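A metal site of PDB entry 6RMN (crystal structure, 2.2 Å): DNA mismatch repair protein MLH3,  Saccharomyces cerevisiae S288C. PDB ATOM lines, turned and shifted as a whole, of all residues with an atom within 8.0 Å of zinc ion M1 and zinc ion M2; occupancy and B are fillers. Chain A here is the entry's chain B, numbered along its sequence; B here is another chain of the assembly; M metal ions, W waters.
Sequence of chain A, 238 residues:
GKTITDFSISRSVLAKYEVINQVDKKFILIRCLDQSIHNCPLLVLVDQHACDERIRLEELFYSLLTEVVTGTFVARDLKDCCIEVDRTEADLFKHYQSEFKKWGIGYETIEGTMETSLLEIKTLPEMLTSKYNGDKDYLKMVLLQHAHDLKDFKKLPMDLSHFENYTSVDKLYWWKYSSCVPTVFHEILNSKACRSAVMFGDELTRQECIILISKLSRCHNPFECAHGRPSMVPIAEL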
ATOM      1  N   ASP A  47       7.252   8.488  -8.094  1.00  0.00           N
ATOM      2  CA  ASP A  47       7.688   7.121  -7.802  1.00  0.00           C
ATOM      3  C   ASP A  47       6.743   6.199  -8.625  1.00  0.00           C
ATOM      4  O   ASP A  47       5.525   6.265  -8.462  1.00  0.00           O
ATOM      5  CB  ASP A  47       7.530   6.866  -6.288  1.00  0.00           C
ATOM      6  CG  ASP A  47       7.903   5.478  -5.759  1.00  0.00           C
ATOM      7  OD1 ASP A  47       7.753   4.489  -6.510  1.00  0.00           O
ATOM      8  OD2 ASP A  47       8.302   5.385  -4.580  1.00  0.00           O
ATOM      9  N   HIS A  49       6.288   2.965  -8.523  1.00  0.00           N
ATOM     10  CA  HIS A  49       5.667   1.934  -7.700  1.00  0.00           C
ATOM     11  C   HIS A  49       4.497   2.527  -6.900  1.00  0.00           C
ATOM     12  O   HIS A  49       3.396   1.972  -6.963  1.00  0.00           O
ATOM     13  CB  HIS A  49       6.714   1.263  -6.787  1.00  0.00           C
ATOM     14  CG  HIS A  49       6.102   0.308  -5.826  1.00  0.00           C
ATOM     15  ND1 HIS A  49       5.610  -0.920  -6.231  1.00  0.00           N
ATOM     16  CD2 HIS A  49       5.838   0.460  -4.510  1.00  0.00           C
ATOM     17  CE1 HIS A  49       5.106  -1.480  -5.151  1.00  0.00           C
ATOM     18  NE2 HIS A  49       5.229  -0.693  -4.101  1.00  0.00           N
ATOM     19  N   ALA A  50       4.727   3.652  -6.206  1.00  0.00           N
ATOM     20  CA  ALA A  50       3.734   4.382  -5.403  1.00  0.00           C
ATOM     21  C   ALA A  50       2.535   4.799  -6.254  1.00  0.00           C
ATOM     22  O   ALA A  50       1.399   4.667  -5.814  1.00  0.00           O
ATOM     23  CB  ALA A  50       4.368   5.602  -4.759  1.00  0.00           C
ATOM     24  N   GLU A  53       0.608   1.484  -7.201  1.00  0.00           N
ATOM     25  CA  GLU A  53       0.028   1.002  -5.942  1.00  0.00           C
ATOM     26  C   GLU A  53      -1.186   1.842  -5.536  1.00  0.00           C
ATOM     27  O   GLU A  53      -2.191   1.276  -5.118  1.00  0.00           O
ATOM     28  CB  GLU A  53       1.094   1.020  -4.837  1.00  0.00           C
ATOM     29  CG  GLU A  53       0.659   0.489  -3.491  1.00  0.00           C
ATOM     30  CD  GLU A  53       1.783   0.585  -2.489  1.00  0.00           C
ATOM     31  OE1 GLU A  53       2.756  -0.194  -2.617  1.00  0.00           O
ATOM     32  OE2 GLU A  53       1.728   1.473  -1.621  1.00  0.00           O
ATOM     33  N   ARG A  54      -1.110   3.181  -5.714  1.00  0.00           N
ATOM     34  CA  ARG A  54      -2.188   4.117  -5.419  1.00  0.00           C
ATOM     35  C   ARG A  54      -3.434   3.860  -6.300  1.00  0.00           C
ATOM     36  O   ARG A  54      -4.560   3.817  -5.777  1.00  0.00           O
ATOM     37  CB  ARG A  54      -1.726   5.565  -5.597  1.00  0.00           C
ATOM     38  CG  ARG A  54      -2.808   6.585  -5.231  1.00  0.00           C
ATOM     39  CD  ARG A  54      -2.910   6.651  -3.736  1.00  0.00           C
ATOM     40  NE  ARG A  54      -4.235   6.342  -3.251  1.00  0.00           N
ATOM     41  CZ  ARG A  54      -4.580   6.368  -1.966  1.00  0.00           C
ATOM     42  NH1 ARG A  54      -3.671   6.658  -1.039  1.00  0.00           N
ATOM     43  NH2 ARG A  54      -5.816   6.088  -1.605  1.00  0.00           N
ATOM     44  N   ASN A 190      -3.990  -3.005   1.088  1.00  0.00           N
ATOM     45  CA  ASN A 190      -2.693  -2.331   0.987  1.00  0.00           C
ATOM     46  C   ASN A 190      -1.635  -3.270   0.470  1.00  0.00           C
ATOM     47  O   ASN A 190      -0.873  -2.864  -0.423  1.00  0.00           O
ATOM     48  CB  ASN A 190      -2.242  -1.743   2.320  1.00  0.00           C
ATOM     49  CG  ASN A 190      -2.900  -0.432   2.679  1.00  0.00           C
ATOM     50  OD1 ASN A 190      -3.747   0.082   1.943  1.00  0.00           O
ATOM     51  ND2 ASN A 190      -2.536   0.120   3.836  1.00  0.00           N
ATOM     52  N   SER A 191      -1.612  -4.512   0.982  1.00  0.00           N
ATOM     53  CA  SER A 191      -0.637  -5.523   0.582  1.00  0.00           C
ATOM     54  C   SER A 191      -0.900  -6.120  -0.785  1.00  0.00           C
ATOM     55  O   SER A 191       0.069  -6.466  -1.466  1.00  0.00           O
ATOM     56  CB  SER A 191      -0.497  -6.609   1.644  1.00  0.00           C
ATOM     57  OG  SER A 191      -1.663  -7.407   1.730  1.00  0.00           O
ATOM     58  N   ALA A 193      -2.331  -4.437  -3.354  1.00  0.00           N
ATOM     59  CA  ALA A 193      -2.001  -3.322  -4.242  1.00  0.00           C
ATOM     60  C   ALA A 193      -0.489  -3.194  -4.389  1.00  0.00           C
ATOM     61  O   ALA A 193      -0.006  -3.094  -5.520  1.00  0.00           O
ATOM     62  CB  ALA A 193      -2.604  -2.024  -3.714  1.00  0.00           C
ATOM     63  N   CYS A 194       0.250  -3.270  -3.265  1.00  0.00           N
ATOM     64  CA  CYS A 194       1.713  -3.227  -3.217  1.00  0.00           C
ATOM     65  C   CYS A 194       2.302  -4.347  -4.082  1.00  0.00           C
ATOM     66  O   CYS A 194       3.115  -4.065  -4.973  1.00  0.00           O
ATOM     67  CB  CYS A 194       2.201  -3.316  -1.772  1.00  0.00           C
ATOM     68  SG  CYS A 194       3.992  -3.125  -1.583  1.00  0.00           S
ATOM     69  N   ARG A 195       1.825  -5.587  -3.888  1.00  0.00           N
ATOM     70  CA  ARG A 195       2.269  -6.766  -4.629  1.00  0.00           C
ATOM     71  C   ARG A 195       1.978  -6.750  -6.111  1.00  0.00           C
ATOM     72  O   ARG A 195       2.750  -7.318  -6.868  1.00  0.00           O
ATOM     73  CB  ARG A 195       1.673  -8.042  -4.020  1.00  0.00           C
ATOM     74  CG  ARG A 195       2.431  -8.518  -2.823  1.00  0.00           C
ATOM     75  CD  ARG A 195       3.456  -9.582  -3.131  1.00  0.00           C
ATOM     76  NE  ARG A 195       3.924 -10.102  -1.850  1.00  0.00           N
ATOM     77  CZ  ARG A 195       3.475 -11.212  -1.279  1.00  0.00           C
ATOM     78  NH1 ARG A 195       2.634 -12.011  -1.917  1.00  0.00           N
ATOM     79  NH2 ARG A 195       3.918 -11.555  -0.070  1.00  0.00           N
ATOM     80  N   SER A 196       0.838  -6.182  -6.516  1.00  0.00           N
ATOM     81  CA  SER A 196       0.441  -6.148  -7.922  1.00  0.00           C
ATOM     82  C   SER A 196       1.142  -5.043  -8.693  1.00  0.00           C
ATOM     83  O   SER A 196       1.249  -5.139  -9.916  1.00  0.00           O
ATOM     84  CB  SER A 196      -1.069  -6.004  -8.037  1.00  0.00           C
ATOM     85  OG  SER A 196      -1.718  -7.212  -7.722  1.00  0.00           O
ATOM     86  N   ALA A 197       1.594  -3.992  -7.982  1.00  0.00           N
ATOM     87  CA  ALA A 197       2.225  -2.812  -8.545  1.00  0.00           C
ATOM     88  C   ALA A 197       3.557  -3.071  -9.188  1.00  0.00           C
ATOM     89  O   ALA A 197       4.285  -3.987  -8.802  1.00  0.00           O
ATOM     90  CB  ALA A 197       2.354  -1.711  -7.497  1.00  0.00           C
ATOM     91  N   VAL A 198       3.892  -2.227 -10.187  1.00  0.00           N
ATOM     92  CA  VAL A 198       5.152  -2.227 -10.911  1.00  0.00           C
ATOM     93  C   VAL A 198       6.251  -1.887  -9.878  1.00  0.00           C
ATOM     94  O   VAL A 198       5.977  -1.182  -8.909  1.00  0.00           O
ATOM     95  CB  VAL A 198       5.075  -1.273 -12.150  1.00  0.00           C
ATOM     96  CG1 VAL A 198       5.147   0.207 -11.783  1.00  0.00           C
ATOM     97  CG2 VAL A 198       6.110  -1.622 -13.195  1.00  0.00           C
ATOM     98  N   MET A 199       7.447  -2.460 -10.040  1.00  0.00           N
ATOM     99  CA  MET A 199       8.541  -2.251  -9.097  1.00  0.00           C
ATOM    100  C   MET A 199       9.660  -1.344  -9.632  1.00  0.00           C
ATOM    101  O   MET A 199       9.714  -1.058 -10.829  1.00  0.00           O
ATOM    102  CB  MET A 199       9.143  -3.614  -8.701  1.00  0.00           C
ATOM    103  CG  MET A 199       8.487  -4.269  -7.508  1.00  0.00           C
ATOM    104  SD  MET A 199       9.330  -5.809  -7.011  1.00  0.00           S
ATOM    105  CE  MET A 199      10.739  -5.143  -6.088  1.00  0.00           C
ATOM    106  N   GLU A 224       0.063  10.209  -2.181  1.00  0.00           N
ATOM    107  CA  GLU A 224       0.746   9.201  -1.368  1.00  0.00           C
ATOM    108  C   GLU A 224       0.458   7.801  -1.861  1.00  0.00           C
ATOM    109  O   GLU A 224      -0.500   7.607  -2.582  1.00  0.00           O
ATOM    110  CB  GLU A 224       0.458   9.359   0.157  1.00  0.00           C
ATOM    111  CG  GLU A 224      -0.979   9.230   0.610  1.00  0.00           C
ATOM    112  CD  GLU A 224      -1.247   9.751   2.012  1.00  0.00           C
ATOM    113  OE1 GLU A 224      -0.885  10.919   2.291  1.00  0.00           O
ATOM    114  OE2 GLU A 224      -1.833   9.008   2.822  1.00  0.00           O
ATOM    115  N   CYS A 225       1.314   6.835  -1.516  1.00  0.00           N
ATOM    116  CA  CYS A 225       1.152   5.413  -1.842  1.00  0.00           C
ATOM    117  C   CYS A 225       0.059   4.837  -0.910  1.00  0.00           C
ATOM    118  O   CYS A 225      -0.518   5.570  -0.085  1.00  0.00           O
ATOM    119  CB  CYS A 225       2.470   4.671  -1.673  1.00  0.00           C
ATOM    120  SG  CYS A 225       2.961   4.425   0.049  1.00  0.00           S
ATOM    121  N   ALA A 226      -0.202   3.503  -1.000  1.00  0.00           N
ATOM    122  CA  ALA A 226      -1.181   2.852  -0.131  1.00  0.00           C
ATOM    123  C   ALA A 226      -0.850   2.978   1.376  1.00  0.00           C
ATOM    124  O   ALA A 226      -1.775   3.124   2.166  1.00  0.00           O
ATOM    125  CB  ALA A 226      -1.359   1.387  -0.503  1.00  0.00           C
ATOM    126  N   HIS A 227       0.460   2.991   1.744  1.00  0.00           N
ATOM    127  CA  HIS A 227       0.971   3.068   3.127  1.00  0.00           C
ATOM    128  C   HIS A 227       1.265   4.490   3.636  1.00  0.00           C
ATOM    129  O   HIS A 227       2.008   4.662   4.604  1.00  0.00           O
ATOM    130  CB  HIS A 227       2.213   2.165   3.276  1.00  0.00           C
ATOM    131  CG  HIS A 227       2.044   0.814   2.647  1.00  0.00           C
ATOM    132  ND1 HIS A 227       2.271   0.616   1.297  1.00  0.00           N
ATOM    133  CD2 HIS A 227       1.595  -0.347   3.189  1.00  0.00           C
ATOM    134  CE1 HIS A 227       1.969  -0.648   1.065  1.00  0.00           C
ATOM    135  NE2 HIS A 227       1.558  -1.269   2.168  1.00  0.00           N
ATOM    136  N   GLY A 228       0.655   5.502   3.012  1.00  0.00           N
ATOM    137  CA  GLY A 228       0.780   6.903   3.394  1.00  0.00           C
ATOM    138  C   GLY A 228       2.079   7.652   3.128  1.00  0.00           C
ATOM    139  O   GLY A 228       2.212   8.788   3.574  1.00  0.00           O
ATOM    140  N   ARG A 229       3.029   7.045   2.394  1.00  0.00           N
ATOM    141  CA  ARG A 229       4.319   7.673   2.041  1.00  0.00           C
ATOM    142  C   ARG A 229       4.164   8.520   0.745  1.00  0.00           C
ATOM    143  O   ARG A 229       3.370   8.111  -0.113  1.00  0.00           O
ATOM    144  CB  ARG A 229       5.427   6.613   1.890  1.00  0.00           C
ATOM    145  CG  ARG A 229       5.693   5.840   3.165  1.00  0.00           C
ATOM    146  CD  ARG A 229       7.106   5.313   3.227  1.00  0.00           C
ATOM    147  NE  ARG A 229       7.367   4.569   4.464  1.00  0.00           N
ATOM    148  CZ  ARG A 229       7.974   5.072   5.534  1.00  0.00           C
ATOM    149  NH1 ARG A 229       8.387   6.332   5.545  1.00  0.00           N
ATOM    150  NH2 ARG A 229       8.172   4.313   6.607  1.00  0.00           N
ATOM    151  N   PRO A 230       4.862   9.673   0.572  1.00  0.00           N
ATOM    152  CA  PRO A 230       4.677  10.489  -0.657  1.00  0.00           C
ATOM    153  C   PRO A 230       4.930   9.753  -1.968  1.00  0.00           C
ATOM    154  O   PRO A 230       5.845   8.930  -2.039  1.00  0.00           O
ATOM    155  CB  PRO A 230       5.654  11.653  -0.471  1.00  0.00           C
ATOM    156  CG  PRO A 230       6.637  11.160   0.517  1.00  0.00           C
ATOM    157  CD  PRO A 230       5.839  10.319   1.467  1.00  0.00           C
ATOM    158  N   ARG B 264      11.691   3.085   1.597  1.00  0.00           N
ATOM    159  CA  ARG B 264      10.772   2.012   1.966  1.00  0.00           C
ATOM    160  C   ARG B 264       9.375   2.432   1.529  1.00  0.00           C
ATOM    161  O   ARG B 264       9.129   3.635   1.365  1.00  0.00           O
ATOM    162  CB  ARG B 264      10.850   1.708   3.468  1.00  0.00           C
ATOM    163  CG  ARG B 264      12.143   1.017   3.897  1.00  0.00           C
ATOM    164  CD  ARG B 264      12.025   0.409   5.290  1.00  0.00           C
ATOM    165  NE  ARG B 264      13.190  -0.409   5.634  1.00  0.00           N
ATOM    166  CZ  ARG B 264      13.281  -1.179   6.714  1.00  0.00           C
ATOM    167  NH1 ARG B 264      14.379  -1.889   6.948  1.00  0.00           N
ATOM    168  NH2 ARG B 264      12.272  -1.245   7.580  1.00  0.00           N
ATOM    169  N   CYS B 265       8.485   1.465   1.287  1.00  0.00           N
ATOM    170  CA  CYS B 265       7.113   1.737   0.847  1.00  0.00           C
ATOM    171  C   CYS B 265       6.216   2.149   2.024  1.00  0.00           C
ATOM    172  O   CYS B 265       6.582   1.891   3.195  1.00  0.00           O
ATOM    173  CB  CYS B 265       6.531   0.553   0.072  1.00  0.00           C
ATOM    174  SG  CYS B 265       5.062   0.941  -0.907  1.00  0.00           S
ATOM    175  OXT CYS B 265       5.157   2.774   1.792  1.00  0.00           O
HETATM  176 ZN    ZN M   1       3.354   2.036  -0.050  1.00  0.00          ZN
HETATM  177 ZN    ZN M   2       4.528  -0.890  -2.093  1.00  0.00          ZN
HETATM  178  O   HOH W   1       7.693  -1.837  -1.975  1.00  0.00           O
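Zinc ion M1 is bound by SG of Cys 265 of chain B, ND1 of His 227, OE2 of Glu 53 and SG of Cys 225.
Zinc ion M1 has four donor atoms within binding distance.
Slightly farther from zinc ion M1 lies OXT of Cys 265 of chain B (2.7 Å).
The side-chain sulfur (SG) of Cys 225 lies close to the backbone NH (N) of Arg 229 (3.5 Å).
O of Cys 225 sits at hydrogen-bond distance from NH1 of Arg 54 (3.5 Å).
The guanidinium group (NE) of Arg 229 lies within salt-bridge range of the chain-end carboxylate (O) of Cys 265 of chain B (3.1 Å).
The side-chain carboxylate (OD1) of Asp 47 sits at hydrogen-bond distance from the backbone NH (N) of His 49.
The backbone carbonyl oxygen of Val 198 lies within hydrogen-bond range of a ring nitrogen (ND1) of His 49, 2.7 Å away.
OE2 of Glu 53 lies close to N of Ala 226 (2.9 Å).
Within 4 Å of zinc ion M2: His 49, Glu 53, Cys 194 and Cys 265 of chain B.
The nearest printed residue that does not touch zinc ion M2 is His 227 (4.1 Å).
OE1 of Glu 53 is bound to zinc ion M2 (2.0 Å).
NE2 of His 49 binds zinc ion M2, 2.1 Å away.
SG of Cys 265 of chain B binds zinc ion M2 (2.2 Å).
Zinc ion M2 is bound by SG of Cys 194, 2.4 Å away.
Merely in contact with zinc ion M1: Ala 226 (3.96 Å).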
